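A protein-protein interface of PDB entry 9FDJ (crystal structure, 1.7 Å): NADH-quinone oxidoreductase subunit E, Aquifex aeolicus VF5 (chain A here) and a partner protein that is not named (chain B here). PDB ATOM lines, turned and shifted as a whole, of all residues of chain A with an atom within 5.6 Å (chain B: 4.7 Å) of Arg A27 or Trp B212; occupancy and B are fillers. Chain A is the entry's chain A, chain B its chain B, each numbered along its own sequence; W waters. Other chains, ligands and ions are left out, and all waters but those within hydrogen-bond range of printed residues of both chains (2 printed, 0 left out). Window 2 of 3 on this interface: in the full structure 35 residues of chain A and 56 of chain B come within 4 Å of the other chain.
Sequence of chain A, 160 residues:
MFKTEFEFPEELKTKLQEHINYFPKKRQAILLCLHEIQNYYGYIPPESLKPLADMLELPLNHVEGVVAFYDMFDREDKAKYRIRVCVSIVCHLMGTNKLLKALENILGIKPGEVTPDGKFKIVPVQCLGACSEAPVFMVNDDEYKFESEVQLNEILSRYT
O of Leu B192 lies within hydrogen-bond range of NE2 of Gln A28 (3.1 Å).
N of Lys A25 is in hydrogen-bond range of OE1 of Gln A28, at 3.2 Å. The backbone NH (N) of Trp B212 sits at hydrogen-bond distance from the side-chain carboxylate (OE2) of Glu B193 (2.8 Å).
Among the printed residues, pairs that only touch across the chains: Arg A27 with Gly B194 (3.4 Å), Lys A25 with Trp B212 (3.5 Å), Arg A27 with Trp B212 (3.6 Å), Ile A30 with Gly B194 (3.6 Å), Arg A27 with Glu B193 (3.7 Å) and Gln A28 with Trp B212 (3.7 Å).
Arg A27 touches three residues of chain B. Of the printed residues of chain B, Ile A30 touches Gly B194 (3.6 Å). Printed residues of chain A within 4 Å of Leu B192: Gln A28 (3.1 Å). Leu B211 touches none of the printed residues of chain A. Of chain A, only Lys A25 (3.5 Å), Arg A27 (3.6 Å) and Gln A28 (3.7 Å) come within 4 Å of Trp B212. The nearest printed residue of chain A that does not touch Gly B194 is Gln A28 (4.5 Å).
Hydrophobic or aromatic side chains of chain B that line the printed part of chain A: Trp B212. Of the 8 printed residues of chain A, 4 touch a printed residue of chain B. Along chain A the printed residues that touch a printed residue of chain B span positions 25 to 30. Among the printed residues, 7 pairs touch across the chains. Among the printed residues, no Asp or Glu carboxylate lies within 4 Å of a Lys or Arg side-chain nitrogen of the other chain.
Water W2 lies within hydrogen-bond range of the backbone carbonyl oxygen of Glu B193 and the guanidinium group of Arg A27. Water W1 bridges OE1 of Gln A28 (2.8 Å) and NE1 of Trp B212 (2.8 Å).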
ATOM      1  N   LYS A  25     -22.163  -5.679  13.958  1.00  0.00           N
ATOM      2  CA  LYS A  25     -22.327  -4.233  13.897  1.00  0.00           C
ATOM      3  C   LYS A  25     -21.096  -3.608  13.240  1.00  0.00           C
ATOM      4  O   LYS A  25     -19.951  -4.028  13.468  1.00  0.00           O
ATOM      5  CB  LYS A  25     -22.560  -3.638  15.292  1.00  0.00           C
ATOM      6  CG  LYS A  25     -23.520  -4.418  16.177  1.00  0.00           C
ATOM      7  CD  LYS A  25     -24.038  -3.634  17.378  1.00  0.00           C
ATOM      8  CE  LYS A  25     -25.021  -4.420  18.194  1.00  0.00           C
ATOM      9  NZ  LYS A  25     -25.557  -3.649  19.322  1.00  0.00           N
ATOM     10  N   LYS A  26     -21.347  -2.584  12.429  1.00  0.00           N
ATOM     11  CA  LYS A  26     -20.318  -1.970  11.611  1.00  0.00           C
ATOM     12  C   LYS A  26     -19.172  -1.445  12.473  1.00  0.00           C
ATOM     13  O   LYS A  26     -18.008  -1.623  12.134  1.00  0.00           O
ATOM     14  CB  LYS A  26     -20.930  -0.794  10.847  1.00  0.00           C
ATOM     15  CG  LYS A  26     -21.917  -1.186   9.770  1.00  0.00           C
ATOM     16  CD  LYS A  26     -22.238   0.002   8.868  1.00  0.00           C
ATOM     17  CE  LYS A  26     -23.023  -0.345   7.642  1.00  0.00           C
ATOM     18  NZ  LYS A  26     -24.386  -0.762   7.966  1.00  0.00           N
ATOM     19  N   ARG A  27     -19.515  -0.790  13.585  1.00  0.00           N
ATOM     20  CA  ARG A  27     -18.523  -0.085  14.376  1.00  0.00           C
ATOM     21  C   ARG A  27     -17.509  -1.046  14.981  1.00  0.00           C
ATOM     22  O   ARG A  27     -16.440  -0.619  15.388  1.00  0.00           O
ATOM     23  CB  ARG A  27     -19.187   0.777  15.451  1.00  0.00           C
ATOM     24  CG  ARG A  27     -19.931   0.041  16.554  1.00  0.00           C
ATOM     25  CD  ARG A  27     -20.803   1.071  17.236  1.00  0.00           C
ATOM     26  NE  ARG A  27     -21.719   0.523  18.234  1.00  0.00           N
ATOM     27  CZ  ARG A  27     -23.005   0.293  18.046  1.00  0.00           C
ATOM     28  NH1 ARG A  27     -23.795   0.165  19.094  1.00  0.00           N
ATOM     29  NH2 ARG A  27     -23.518   0.270  16.832  1.00  0.00           N
ATOM     30  N   GLN A  28     -17.834  -2.342  15.047  1.00  0.00           N
ATOM     31  CA  GLN A  28     -16.910  -3.301  15.610  1.00  0.00           C
ATOM     32  C   GLN A  28     -15.689  -3.472  14.719  1.00  0.00           C
ATOM     33  O   GLN A  28     -14.657  -3.955  15.194  1.00  0.00           O
ATOM     34  CB  GLN A  28     -17.544  -4.665  15.858  1.00  0.00           C
ATOM     35  CG  GLN A  28     -18.794  -4.585  16.715  1.00  0.00           C
ATOM     36  CD  GLN A  28     -19.342  -5.954  17.020  1.00  0.00           C
ATOM     37  OE1 GLN A  28     -20.326  -6.391  16.419  1.00  0.00           O
ATOM     38  NE2 GLN A  28     -18.708  -6.628  17.963  1.00  0.00           N
ATOM     39  N   ALA A  29     -15.803  -3.069  13.445  1.00  0.00           N
ATOM     40  CA  ALA A  29     -14.732  -3.269  12.474  1.00  0.00           C
ATOM     41  C   ALA A  29     -13.662  -2.174  12.514  1.00  0.00           C
ATOM     42  O   ALA A  29     -12.746  -2.203  11.699  1.00  0.00           O
ATOM     43  CB  ALA A  29     -15.333  -3.357  11.094  1.00  0.00           C
ATOM     44  N   ILE A  30     -13.758  -1.209  13.442  1.00  0.00           N
ATOM     45  CA  ILE A  30     -12.889  -0.034  13.402  1.00  0.00           C
ATOM     46  C   ILE A  30     -11.393  -0.394  13.413  1.00  0.00           C
ATOM     47  O   ILE A  30     -10.615   0.200  12.661  1.00  0.00           O
ATOM     48  CB  ILE A  30     -13.234   0.982  14.508  1.00  0.00           C
ATOM     49  CG1 ILE A  30     -12.399   2.264  14.345  1.00  0.00           C
ATOM     50  CG2 ILE A  30     -13.082   0.379  15.909  1.00  0.00           C
ATOM     51  CD1 ILE A  30     -12.914   3.439  15.148  1.00  0.00           C
ATOM     52  N   LEU A  56     -18.198   3.640   8.931  1.00  0.00           N
ATOM     53  CA  LEU A  56     -18.444   3.010  10.221  1.00  0.00           C
ATOM     54  C   LEU A  56     -19.718   3.556  10.875  1.00  0.00           C
ATOM     55  O   LEU A  56     -20.148   3.018  11.892  1.00  0.00           O
ATOM     56  CB  LEU A  56     -17.224   3.253  11.115  1.00  0.00           C
ATOM     57  CG  LEU A  56     -15.917   2.541  10.731  1.00  0.00           C
ATOM     58  CD1 LEU A  56     -14.721   3.031  11.533  1.00  0.00           C
ATOM     59  CD2 LEU A  56     -16.053   1.041  10.909  1.00  0.00           C
ATOM     60  N   LEU A  58     -19.788   6.433  12.437  1.00  0.00           N
ATOM     61  CA  LEU A  58     -19.255   6.923  13.701  1.00  0.00           C
ATOM     62  C   LEU A  58     -18.863   8.391  13.551  1.00  0.00           C
ATOM     63  O   LEU A  58     -18.460   8.820  12.477  1.00  0.00           O
ATOM     64  CB  LEU A  58     -18.035   6.105  14.125  1.00  0.00           C
ATOM     65  CG  LEU A  58     -18.307   4.694  14.651  1.00  0.00           C
ATOM     66  CD1 LEU A  58     -16.981   4.035  14.995  1.00  0.00           C
ATOM     67  CD2 LEU A  58     -19.234   4.690  15.859  1.00  0.00           C
ATOM     68  N   TYR B  88     -23.020 -14.014  25.318  1.00  0.00           N
ATOM     69  CA  TYR B  88     -21.890 -13.998  24.419  1.00  0.00           C
ATOM     70  C   TYR B  88     -20.722 -14.710  25.084  1.00  0.00           C
ATOM     71  O   TYR B  88     -20.568 -14.656  26.296  1.00  0.00           O
ATOM     72  CB  TYR B  88     -21.460 -12.565  24.088  1.00  0.00           C
ATOM     73  CG  TYR B  88     -22.540 -11.780  23.354  1.00  0.00           C
ATOM     74  CD1 TYR B  88     -22.949 -12.152  22.076  1.00  0.00           C
ATOM     75  CD2 TYR B  88     -23.146 -10.681  23.939  1.00  0.00           C
ATOM     76  CE1 TYR B  88     -23.937 -11.446  21.399  1.00  0.00           C
ATOM     77  CE2 TYR B  88     -24.127  -9.964  23.277  1.00  0.00           C
ATOM     78  CZ  TYR B  88     -24.528 -10.350  22.007  1.00  0.00           C
ATOM     79  OH  TYR B  88     -25.509  -9.643  21.356  1.00  0.00           O
ATOM     80  N   LEU B 192     -14.105  -4.466  21.601  1.00  0.00           N
ATOM     81  CA  LEU B 192     -14.994  -5.229  20.727  1.00  0.00           C
ATOM     82  C   LEU B 192     -16.177  -4.380  20.272  1.00  0.00           C
ATOM     83  O   LEU B 192     -16.759  -4.634  19.213  1.00  0.00           O
ATOM     84  CB  LEU B 192     -15.517  -6.486  21.412  1.00  0.00           C
ATOM     85  CG  LEU B 192     -14.638  -7.730  21.359  1.00  0.00           C
ATOM     86  CD1 LEU B 192     -15.326  -8.836  22.156  1.00  0.00           C
ATOM     87  CD2 LEU B 192     -14.362  -8.168  19.913  1.00  0.00           C
ATOM     88  N   GLU B 193     -16.566  -3.416  21.105  1.00  0.00           N
ATOM     89  CA  GLU B 193     -17.676  -2.526  20.811  1.00  0.00           C
ATOM     90  C   GLU B 193     -17.215  -1.347  19.949  1.00  0.00           C
ATOM     91  O   GLU B 193     -18.011  -0.453  19.635  1.00  0.00           O
ATOM     92  CB  GLU B 193     -18.321  -2.072  22.123  1.00  0.00           C
ATOM     93  CG  GLU B 193     -19.147  -3.141  22.833  1.00  0.00           C
ATOM     94  CD  GLU B 193     -19.794  -2.706  24.148  1.00  0.00           C
ATOM     95  OE1 GLU B 193     -19.590  -1.543  24.558  1.00  0.00           O
ATOM     96  OE2 GLU B 193     -20.498  -3.513  24.790  1.00  0.00           O
ATOM     97  N   GLY B 194     -15.931  -1.331  19.575  1.00  0.00           N
ATOM     98  CA  GLY B 194     -15.413  -0.344  18.636  1.00  0.00           C
ATOM     99  C   GLY B 194     -14.945   0.932  19.327  1.00  0.00           C
ATOM    100  O   GLY B 194     -14.846   1.970  18.680  1.00  0.00           O
ATOM    101  N   GLY B 210     -22.106  -7.432  30.006  1.00  0.00           N
ATOM    102  CA  GLY B 210     -20.874  -7.500  29.245  1.00  0.00           C
ATOM    103  C   GLY B 210     -21.034  -6.840  27.875  1.00  0.00           C
ATOM    104  O   GLY B 210     -21.347  -5.655  27.794  1.00  0.00           O
ATOM    105  N   LEU B 211     -20.819  -7.625  26.808  1.00  0.00           N
ATOM    106  CA  LEU B 211     -20.928  -7.118  25.446  1.00  0.00           C
ATOM    107  C   LEU B 211     -22.363  -6.688  25.163  1.00  0.00           C
ATOM    108  O   LEU B 211     -23.285  -7.468  25.349  1.00  0.00           O
ATOM    109  CB  LEU B 211     -20.456  -8.194  24.477  1.00  0.00           C
ATOM    110  CG  LEU B 211     -20.414  -7.800  22.997  1.00  0.00           C
ATOM    111  CD1 LEU B 211     -19.404  -6.693  22.723  1.00  0.00           C
ATOM    112  CD2 LEU B 211     -20.112  -9.005  22.141  1.00  0.00           C
ATOM    113  N   TRP B 212     -22.533  -5.427  24.758  1.00  0.00           N
ATOM    114  CA  TRP B 212     -23.842  -4.839  24.508  1.00  0.00           C
ATOM    115  C   TRP B 212     -24.738  -4.961  25.739  1.00  0.00           C
ATOM    116  O   TRP B 212     -25.956  -4.949  25.613  1.00  0.00           O
ATOM    117  CB  TRP B 212     -24.499  -5.465  23.261  1.00  0.00           C
ATOM    118  CG  TRP B 212     -23.599  -5.500  22.049  1.00  0.00           C
ATOM    119  CD1 TRP B 212     -23.316  -6.595  21.285  1.00  0.00           C
ATOM    120  CD2 TRP B 212     -22.872  -4.406  21.445  1.00  0.00           C
ATOM    121  NE1 TRP B 212     -22.454  -6.272  20.273  1.00  0.00           N
ATOM    122  CE2 TRP B 212     -22.166  -4.940  20.341  1.00  0.00           C
ATOM    123  CE3 TRP B 212     -22.733  -3.048  21.732  1.00  0.00           C
ATOM    124  CZ2 TRP B 212     -21.348  -4.160  19.525  1.00  0.00           C
ATOM    125  CZ3 TRP B 212     -21.932  -2.278  20.920  1.00  0.00           C
ATOM    126  CH2 TRP B 212     -21.239  -2.831  19.843  1.00  0.00           C
ATOM    127  N   GLY B 213     -24.120  -5.030  26.927  1.00  0.00           N
ATOM    128  CA  GLY B 213     -24.828  -5.066  28.192  1.00  0.00           C
ATOM    129  C   GLY B 213     -25.414  -6.439  28.517  1.00  0.00           C
ATOM    130  O   GLY B 213     -26.175  -6.569  29.469  1.00  0.00           O
ATOM    131  N   LYS B 214     -25.076  -7.453  27.717  1.00  0.00           N
ATOM    132  CA  LYS B 214     -25.665  -8.774  27.862  1.00  0.00           C
ATOM    133  C   LYS B 214     -24.712  -9.692  28.622  1.00  0.00           C
ATOM    134  O   LYS B 214     -23.501  -9.480  28.608  1.00  0.00           O
ATOM    135  CB  LYS B 214     -25.958  -9.362  26.484  1.00  0.00           C
ATOM    136  CG  LYS B 214     -26.913  -8.517  25.628  1.00  0.00           C
ATOM    137  CD  LYS B 214     -28.257  -8.176  26.258  1.00  0.00           C
ATOM    138  CE  LYS B 214     -29.022  -9.368  26.746  1.00  0.00           C
ATOM    139  NZ  LYS B 214     -30.455  -9.066  26.914  1.00  0.00           N
HETATM  140  O   HOH W   1     -22.088  -7.852  17.975  1.00  0.00           O
HETATM  141  O   HOH W   2     -20.038   1.102  20.424  1.00  0.00           O
